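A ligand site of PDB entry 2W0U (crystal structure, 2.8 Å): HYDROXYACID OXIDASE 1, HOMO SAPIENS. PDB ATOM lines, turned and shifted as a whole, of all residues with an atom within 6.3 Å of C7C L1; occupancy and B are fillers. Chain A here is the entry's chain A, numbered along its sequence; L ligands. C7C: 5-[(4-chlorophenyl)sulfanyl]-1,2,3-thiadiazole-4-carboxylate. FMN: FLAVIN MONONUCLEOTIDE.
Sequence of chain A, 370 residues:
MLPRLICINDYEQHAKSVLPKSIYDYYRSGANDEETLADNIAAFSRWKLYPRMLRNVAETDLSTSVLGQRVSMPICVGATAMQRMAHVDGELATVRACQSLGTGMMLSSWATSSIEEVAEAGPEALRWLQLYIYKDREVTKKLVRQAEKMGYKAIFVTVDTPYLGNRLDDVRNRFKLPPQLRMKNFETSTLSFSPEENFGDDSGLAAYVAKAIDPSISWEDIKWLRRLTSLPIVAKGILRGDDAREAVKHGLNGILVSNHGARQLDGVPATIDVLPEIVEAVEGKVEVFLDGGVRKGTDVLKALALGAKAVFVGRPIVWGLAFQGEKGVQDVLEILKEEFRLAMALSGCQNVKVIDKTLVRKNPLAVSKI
O of Tyr 26 lies within hydrogen-bond range of NH1 of Arg 263, 2.9 Å away.
O of Arg 263 sits at hydrogen-bond distance from NE of Arg 167 (3.0 Å).
The backbone carbonyl oxygen (O) of Trp 110 lies within hydrogen-bond range of the backbone NH (N) of Met 82.
OG1 of Thr 161 sits close to ND1 of His 260, at 3.2 Å.
The guanidinium group of Arg 167 is in hydrogen-bond range of the side-chain amide oxygen of Gln 264.
Merely in contact with C7C L1: Met 82 (3.7 Å), Trp 110 (2.7 Å), Leu 205 (3.8 Å), Tyr 208 (3.7 Å) and Val 209 (3.9 Å).
Hydrophobic or aromatic side chains within 4 Å of C7C L1: Tyr 26, Met 82, Trp 110, Tyr 132, Leu 205, Tyr 208, Val 209 and His 260.
NE of Arg 263 is in salt-bridge range of O16 of C7C L1.
N11 of C7C L1 lies within hydrogen-bond range of OH of Tyr 132.
A ring nitrogen (NE2) of His 260 sits at hydrogen-bond distance from a nitrogen (N12) of C7C L1, 2.9 Å away.
The side-chain hydroxyl (OH) of Tyr 26 is in hydrogen-bond range of an oxygen (O15) of C7C L1, at 3.1 Å.
The guanidinium group of Arg 167 is in salt-bridge range of an oxygen (O16) of C7C L1, 3.3 Å away.
N3 of FMN L2 is in hydrogen-bond range of OH of Tyr 132, at 3.5 Å.
A nitrogen (N1) of FMN L2 is in hydrogen-bond range of a ring nitrogen (NE2) of His 260 (3.4 Å).
A nitrogen (N5) of FMN L2 lies within hydrogen-bond range of the backbone NH (N) of Ala 81 (3.4 Å).
OG of Ser 109 lies within hydrogen-bond range of O4 of FMN L2 (3.5 Å).
N3 of FMN L2 lies within hydrogen-bond range of OE1 of Gln 130 (2.9 Å).
OG of Ser 108 is in hydrogen-bond range of O4 of FMN L2 (2.8 Å).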
ATOM      1  N   TYR A  26      12.697  -8.011   5.470  1.00  0.00           N
ATOM      2  CA  TYR A  26      13.965  -8.540   5.963  1.00  0.00           C
ATOM      3  C   TYR A  26      14.612  -9.517   4.959  1.00  0.00           C
ATOM      4  O   TYR A  26      15.828  -9.455   4.728  1.00  0.00           O
ATOM      5  CB  TYR A  26      13.809  -9.191   7.342  1.00  0.00           C
ATOM      6  CG  TYR A  26      14.909 -10.188   7.610  1.00  0.00           C
ATOM      7  CD1 TYR A  26      16.201  -9.761   7.924  1.00  0.00           C
ATOM      8  CD2 TYR A  26      14.684 -11.549   7.466  1.00  0.00           C
ATOM      9  CE1 TYR A  26      17.220 -10.670   8.127  1.00  0.00           C
ATOM     10  CE2 TYR A  26      15.693 -12.457   7.671  1.00  0.00           C
ATOM     11  CZ  TYR A  26      16.958 -12.016   7.991  1.00  0.00           C
ATOM     12  OH  TYR A  26      17.958 -12.922   8.200  1.00  0.00           O
ATOM     13  N   ALA A  81      19.655 -17.043   7.238  1.00  0.00           N
ATOM     14  CA  ALA A  81      19.329 -17.103   8.662  1.00  0.00           C
ATOM     15  C   ALA A  81      17.831 -17.109   8.917  1.00  0.00           C
ATOM     16  O   ALA A  81      17.056 -16.610   8.093  1.00  0.00           O
ATOM     17  CB  ALA A  81      19.970 -15.937   9.386  1.00  0.00           C
ATOM     18  N   MET A  82      17.431 -17.690  10.041  1.00  0.00           N
ATOM     19  CA  MET A  82      16.083 -17.594  10.597  1.00  0.00           C
ATOM     20  C   MET A  82      14.980 -18.023   9.633  1.00  0.00           C
ATOM     21  O   MET A  82      14.078 -17.241   9.304  1.00  0.00           O
ATOM     22  CB  MET A  82      15.820 -16.179  11.107  1.00  0.00           C
ATOM     23  CG  MET A  82      16.942 -15.620  11.962  1.00  0.00           C
ATOM     24  SD  MET A  82      16.470 -14.059  12.697  1.00  0.00           S
ATOM     25  CE  MET A  82      16.490 -12.938  11.301  1.00  0.00           C
ATOM     26  N   SER A 108      22.885 -22.253   7.758  1.00  0.00           N
ATOM     27  CA  SER A 108      23.292 -20.904   8.072  1.00  0.00           C
ATOM     28  C   SER A 108      23.639 -20.750   9.541  1.00  0.00           C
ATOM     29  O   SER A 108      23.210 -21.525  10.393  1.00  0.00           O
ATOM     30  CB  SER A 108      22.192 -19.928   7.687  1.00  0.00           C
ATOM     31  OG  SER A 108      22.580 -18.612   8.053  1.00  0.00           O
ATOM     32  N   SER A 109      24.438 -19.732   9.825  1.00  0.00           N
ATOM     33  CA  SER A 109      24.600 -19.259  11.178  1.00  0.00           C
ATOM     34  C   SER A 109      23.290 -18.558  11.557  1.00  0.00           C
ATOM     35  O   SER A 109      22.556 -18.100  10.686  1.00  0.00           O
ATOM     36  CB  SER A 109      25.782 -18.301  11.264  1.00  0.00           C
ATOM     37  OG  SER A 109      25.617 -17.225  10.362  1.00  0.00           O
ATOM     38  N   TRP A 110      23.011 -18.493  12.864  1.00  0.00           N
ATOM     39  CA  TRP A 110      21.728 -17.994  13.368  1.00  0.00           C
ATOM     40  C   TRP A 110      20.544 -18.740  12.748  1.00  0.00           C
ATOM     41  O   TRP A 110      19.508 -18.146  12.468  1.00  0.00           O
ATOM     42  CB  TRP A 110      21.569 -16.496  13.155  1.00  0.00           C
ATOM     43  CG  TRP A 110      22.269 -15.682  14.179  1.00  0.00           C
ATOM     44  CD1 TRP A 110      21.851 -15.448  15.460  1.00  0.00           C
ATOM     45  CD2 TRP A 110      23.507 -14.985  14.028  1.00  0.00           C
ATOM     46  NE1 TRP A 110      22.766 -14.644  16.110  1.00  0.00           N
ATOM     47  CE2 TRP A 110      23.785 -14.341  15.254  1.00  0.00           C
ATOM     48  CE3 TRP A 110      24.418 -14.837  12.963  1.00  0.00           C
ATOM     49  CZ2 TRP A 110      24.916 -13.566  15.445  1.00  0.00           C
ATOM     50  CZ3 TRP A 110      25.539 -14.070  13.161  1.00  0.00           C
ATOM     51  CH2 TRP A 110      25.784 -13.442  14.395  1.00  0.00           C
ATOM     52  N   GLN A 130      27.735 -23.138   7.320  1.00  0.00           N
ATOM     53  CA  GLN A 130      28.228 -21.777   7.212  1.00  0.00           C
ATOM     54  C   GLN A 130      28.476 -21.261   8.608  1.00  0.00           C
ATOM     55  O   GLN A 130      27.694 -21.500   9.529  1.00  0.00           O
ATOM     56  CB  GLN A 130      27.248 -20.869   6.453  1.00  0.00           C
ATOM     57  CG  GLN A 130      27.768 -19.445   6.200  1.00  0.00           C
ATOM     58  CD  GLN A 130      27.402 -18.477   7.311  1.00  0.00           C
ATOM     59  OE1 GLN A 130      26.285 -18.479   7.809  1.00  0.00           O
ATOM     60  NE2 GLN A 130      28.346 -17.656   7.718  1.00  0.00           N
ATOM     61  N   TYR A 132      30.839 -18.089  11.091  1.00  0.00           N
ATOM     62  CA  TYR A 132      31.690 -16.915  11.255  1.00  0.00           C
ATOM     63  C   TYR A 132      32.751 -17.243  12.269  1.00  0.00           C
ATOM     64  O   TYR A 132      32.550 -18.116  13.121  1.00  0.00           O
ATOM     65  CB  TYR A 132      30.894 -15.718  11.758  1.00  0.00           C
ATOM     66  CG  TYR A 132      29.923 -15.153  10.763  1.00  0.00           C
ATOM     67  CD1 TYR A 132      30.371 -14.424   9.671  1.00  0.00           C
ATOM     68  CD2 TYR A 132      28.552 -15.331  10.914  1.00  0.00           C
ATOM     69  CE1 TYR A 132      29.480 -13.894   8.769  1.00  0.00           C
ATOM     70  CE2 TYR A 132      27.661 -14.801  10.012  1.00  0.00           C
ATOM     71  CZ  TYR A 132      28.133 -14.088   8.938  1.00  0.00           C
ATOM     72  OH  TYR A 132      27.251 -13.569   8.037  1.00  0.00           O
ATOM     73  N   THR A 161      31.727  -9.919   6.386  1.00  0.00           N
ATOM     74  CA  THR A 161      30.843  -9.305   7.382  1.00  0.00           C
ATOM     75  C   THR A 161      31.547  -8.979   8.707  1.00  0.00           C
ATOM     76  O   THR A 161      31.156  -9.481   9.756  1.00  0.00           O
ATOM     77  CB  THR A 161      29.583 -10.190   7.629  1.00  0.00           C
ATOM     78  OG1 THR A 161      29.089 -10.682   6.379  1.00  0.00           O
ATOM     79  CG2 THR A 161      28.482  -9.405   8.303  1.00  0.00           C
ATOM     80  N   LEU A 164      27.653  -5.857  10.281  1.00  0.00           N
ATOM     81  CA  LEU A 164      26.471  -6.109   9.469  1.00  0.00           C
ATOM     82  C   LEU A 164      26.161  -4.923   8.553  1.00  0.00           C
ATOM     83  O   LEU A 164      26.346  -3.759   8.939  1.00  0.00           O
ATOM     84  CB  LEU A 164      25.269  -6.423  10.355  1.00  0.00           C
ATOM     85  CG  LEU A 164      24.056  -7.060   9.653  1.00  0.00           C
ATOM     86  CD1 LEU A 164      24.249  -8.567   9.495  1.00  0.00           C
ATOM     87  CD2 LEU A 164      22.781  -6.765  10.417  1.00  0.00           C
ATOM     88  N   ARG A 167      20.801  -2.114   6.063  1.00  0.00           N
ATOM     89  CA  ARG A 167      19.592  -2.395   5.282  1.00  0.00           C
ATOM     90  C   ARG A 167      18.474  -1.476   5.736  1.00  0.00           C
ATOM     91  O   ARG A 167      17.903  -1.669   6.817  1.00  0.00           O
ATOM     92  CB  ARG A 167      19.197  -3.867   5.423  1.00  0.00           C
ATOM     93  CG  ARG A 167      20.186  -4.841   4.802  1.00  0.00           C
ATOM     94  CD  ARG A 167      20.335  -6.104   5.627  1.00  0.00           C
ATOM     95  NE  ARG A 167      21.669  -6.680   5.478  1.00  0.00           N
ATOM     96  CZ  ARG A 167      22.214  -7.572   6.302  1.00  0.00           C
ATOM     97  NH1 ARG A 167      21.527  -8.003   7.353  1.00  0.00           N
ATOM     98  NH2 ARG A 167      23.437  -8.039   6.081  1.00  0.00           N
ATOM     99  N   LEU A 205      19.213  -5.722  14.672  1.00  0.00           N
ATOM    100  CA  LEU A 205      20.049  -6.882  14.333  1.00  0.00           C
ATOM    101  C   LEU A 205      21.554  -6.567  14.286  1.00  0.00           C
ATOM    102  O   LEU A 205      22.381  -7.457  14.512  1.00  0.00           O
ATOM    103  CB  LEU A 205      19.603  -7.501  13.006  1.00  0.00           C
ATOM    104  CG  LEU A 205      18.316  -8.332  12.986  1.00  0.00           C
ATOM    105  CD1 LEU A 205      17.931  -8.651  11.555  1.00  0.00           C
ATOM    106  CD2 LEU A 205      18.444  -9.622  13.795  1.00  0.00           C
ATOM    107  N   ALA A 206      21.891  -5.317  13.995  1.00  0.00           N
ATOM    108  CA  ALA A 206      23.291  -4.879  13.857  1.00  0.00           C
ATOM    109  C   ALA A 206      24.087  -4.960  15.161  1.00  0.00           C
ATOM    110  O   ALA A 206      25.308  -5.143  15.137  1.00  0.00           O
ATOM    111  CB  ALA A 206      23.364  -3.468  13.266  1.00  0.00           C
ATOM    112  N   TYR A 208      23.593  -7.300  17.703  1.00  0.00           N
ATOM    113  CA  TYR A 208      23.852  -8.716  17.950  1.00  0.00           C
ATOM    114  C   TYR A 208      25.083  -9.218  17.197  1.00  0.00           C
ATOM    115  O   TYR A 208      25.821 -10.082  17.686  1.00  0.00           O
ATOM    116  CB  TYR A 208      22.641  -9.560  17.556  1.00  0.00           C
ATOM    117  CG  TYR A 208      21.617  -9.762  18.661  1.00  0.00           C
ATOM    118  CD1 TYR A 208      21.758 -10.812  19.574  1.00  0.00           C
ATOM    119  CD2 TYR A 208      20.510  -8.924  18.777  1.00  0.00           C
ATOM    120  CE1 TYR A 208      20.824 -11.016  20.599  1.00  0.00           C
ATOM    121  CE2 TYR A 208      19.565  -9.110  19.789  1.00  0.00           C
ATOM    122  CZ  TYR A 208      19.734 -10.165  20.693  1.00  0.00           C
ATOM    123  OH  TYR A 208      18.807 -10.355  21.699  1.00  0.00           O
ATOM    124  N   VAL A 209      25.286  -8.689  15.988  1.00  0.00           N
ATOM    125  CA  VAL A 209      26.426  -9.040  15.139  1.00  0.00           C
ATOM    126  C   VAL A 209      27.724  -8.484  15.722  1.00  0.00           C
ATOM    127  O   VAL A 209      28.747  -9.177  15.758  1.00  0.00           O
ATOM    128  CB  VAL A 209      26.221  -8.536  13.682  1.00  0.00           C
ATOM    129  CG1 VAL A 209      27.419  -8.859  12.800  1.00  0.00           C
ATOM    130  CG2 VAL A 209      24.955  -9.121  13.084  1.00  0.00           C
ATOM    131  N   ILE A 213      30.318 -11.241  16.240  1.00  0.00           N
ATOM    132  CA  ILE A 213      31.276 -11.346  15.131  1.00  0.00           C
ATOM    133  C   ILE A 213      32.457 -10.414  15.293  1.00  0.00           C
ATOM    134  O   ILE A 213      32.292  -9.218  15.479  1.00  0.00           O
ATOM    135  CB  ILE A 213      30.598 -11.137  13.759  1.00  0.00           C
ATOM    136  CG1 ILE A 213      29.421 -12.101  13.594  1.00  0.00           C
ATOM    137  CG2 ILE A 213      31.632 -11.325  12.636  1.00  0.00           C
ATOM    138  CD1 ILE A 213      28.640 -11.945  12.326  1.00  0.00           C
ATOM    139  N   HIS A 260      26.965 -11.516  -0.621  1.00  0.00           N
ATOM    140  CA  HIS A 260      26.114 -11.704   0.547  1.00  0.00           C
ATOM    141  C   HIS A 260      24.667 -11.340   0.215  1.00  0.00           C
ATOM    142  O   HIS A 260      23.978 -10.747   1.040  1.00  0.00           O
ATOM    143  CB  HIS A 260      26.653 -10.870   1.719  1.00  0.00           C
ATOM    144  CG  HIS A 260      26.289 -11.389   3.078  1.00  0.00           C
ATOM    145  ND1 HIS A 260      27.231 -11.816   3.980  1.00  0.00           N
ATOM    146  CD2 HIS A 260      25.089 -11.527   3.689  1.00  0.00           C
ATOM    147  CE1 HIS A 260      26.636 -12.208   5.095  1.00  0.00           C
ATOM    148  NE2 HIS A 260      25.341 -12.044   4.940  1.00  0.00           N
ATOM    149  N   ARG A 263      23.596  -7.578   0.523  1.00  0.00           N
ATOM    150  CA  ARG A 263      23.147  -7.133   1.823  1.00  0.00           C
ATOM    151  C   ARG A 263      24.249  -6.429   2.636  1.00  0.00           C
ATOM    152  O   ARG A 263      23.968  -5.864   3.705  1.00  0.00           O
ATOM    153  CB  ARG A 263      22.556  -8.311   2.595  1.00  0.00           C
ATOM    154  CG  ARG A 263      21.254  -8.808   1.970  1.00  0.00           C
ATOM    155  CD  ARG A 263      20.921 -10.206   2.354  1.00  0.00           C
ATOM    156  NE  ARG A 263      20.391 -10.323   3.709  1.00  0.00           N
ATOM    157  CZ  ARG A 263      19.105 -10.202   4.052  1.00  0.00           C
ATOM    158  NH1 ARG A 263      18.188  -9.927   3.146  1.00  0.00           N
ATOM    159  NH2 ARG A 263      18.743 -10.350   5.317  1.00  0.00           N
ATOM    160  N   GLN A 264      25.478  -6.455   2.137  1.00  0.00           N
ATOM    161  CA  GLN A 264      26.616  -5.914   2.857  1.00  0.00           C
ATOM    162  C   GLN A 264      27.054  -4.526   2.344  1.00  0.00           C
ATOM    163  O   GLN A 264      26.482  -3.515   2.754  1.00  0.00           O
ATOM    164  CB  GLN A 264      27.776  -6.906   2.885  1.00  0.00           C
ATOM    165  CG  GLN A 264      27.546  -8.070   3.837  1.00  0.00           C
ATOM    166  CD  GLN A 264      27.311  -7.632   5.269  1.00  0.00           C
ATOM    167  OE1 GLN A 264      26.214  -7.789   5.813  1.00  0.00           O
ATOM    168  NE2 GLN A 264      28.339  -7.055   5.896  1.00  0.00           N
HETATM  169 CL   C7C L   1      21.108 -12.521  16.071  1.00  0.00          CL
HETATM  170  C1  C7C L   1      21.023 -12.301  14.292  1.00  0.00           C
HETATM  171  C2  C7C L   1      20.161 -13.093  13.538  1.00  0.00           C
HETATM  172  C3  C7C L   1      20.095 -12.919  12.162  1.00  0.00           C
HETATM  173  C6  C7C L   1      21.816 -11.348  13.664  1.00  0.00           C
HETATM  174  C5  C7C L   1      21.749 -11.183  12.291  1.00  0.00           C
HETATM  175  C4  C7C L   1      20.888 -11.966  11.534  1.00  0.00           C
HETATM  176  S8  C7C L   1      20.800 -11.763   9.852  1.00  0.00           S
HETATM  177  C9  C7C L   1      22.332 -12.213   9.142  1.00  0.00           C
HETATM  178  C13 C7C L   1      22.674 -12.050   7.710  1.00  0.00           C
HETATM  179  C14 C7C L   1      21.685 -11.480   6.754  1.00  0.00           C
HETATM  180  O15 C7C L   1      20.486 -11.435   7.077  1.00  0.00           O
HETATM  181  O16 C7C L   1      22.096 -11.054   5.645  1.00  0.00           O
HETATM  182  S10 C7C L   1      23.657 -12.906   9.985  1.00  0.00           S
HETATM  183  N11 C7C L   1      24.646 -13.002   8.612  1.00  0.00           N
HETATM  184  N12 C7C L   1      23.948 -12.504   7.476  1.00  0.00           N
HETATM  185  N1  FMN L   2      25.137 -15.405   4.253  1.00  0.00           N
HETATM  186  C2  FMN L   2      25.913 -15.899   5.267  1.00  0.00           C
HETATM  187  O2  FMN L   2      27.090 -16.177   5.033  1.00  0.00           O
HETATM  188  N3  FMN L   2      25.384 -16.072   6.528  1.00  0.00           N
HETATM  189  C4  FMN L   2      24.057 -15.759   6.775  1.00  0.00           C
HETATM  190  O4  FMN L   2      23.573 -15.946   7.888  1.00  0.00           O
HETATM  191  C4A FMN L   2      23.266 -15.270   5.747  1.00  0.00           C
HETATM  192  N5  FMN L   2      21.955 -14.954   5.976  1.00  0.00           N
HETATM  193  C5A FMN L   2      21.167 -14.462   4.956  1.00  0.00           C
HETATM  194  C6  FMN L   2      19.828 -14.141   5.194  1.00  0.00           C
HETATM  195  C7  FMN L   2      19.014 -13.651   4.163  1.00  0.00           C
HETATM  196  C7M FMN L   2      17.531 -13.647   4.330  1.00  0.00           C
HETATM  197  C8  FMN L   2      19.557 -13.485   2.887  1.00  0.00           C
HETATM  198  C8M FMN L   2      18.680 -13.077   1.740  1.00  0.00           C
HETATM  199  C9  FMN L   2      20.901 -13.793   2.655  1.00  0.00           C
HETATM  200  C9A FMN L   2      21.705 -14.281   3.689  1.00  0.00           C
HETATM  201  N10 FMN L   2      23.025 -14.599   3.457  1.00  0.00           N
HETATM  202  C10 FMN L   2      23.814 -15.091   4.477  1.00  0.00           C
HETATM  203  C1' FMN L   2      23.577 -14.529   2.064  1.00  0.00           C
HETATM  204  C2' FMN L   2      23.321 -15.840   1.351  1.00  0.00           C
HETATM  205  O2' FMN L   2      24.165 -16.835   1.877  1.00  0.00           O
HETATM  206  C3' FMN L   2      23.591 -15.735  -0.135  1.00  0.00           C
HETATM  207  O3' FMN L   2      24.843 -15.118  -0.298  1.00  0.00           O
HETATM  208  C4' FMN L   2      22.569 -14.898  -0.887  1.00  0.00           C
HETATM  209  O4' FMN L   2      21.280 -15.118  -0.370  1.00  0.00           O
HETATM  210  C5' FMN L   2      22.588 -15.274  -2.356  1.00  0.00           C
HETATM  211  O5' FMN L   2      21.800 -14.347  -3.062  1.00  0.00           O
HETATM  212  P   FMN L   2      20.289 -14.690  -3.499  1.00  0.00           P
HETATM  213  O1P FMN L   2      19.929 -13.749  -4.627  1.00  0.00           O
HETATM  214  O2P FMN L   2      19.372 -14.504  -2.309  1.00  0.00           O
HETATM  215  O3P FMN L   2      20.179 -16.104  -3.976  1.00  0.00           O
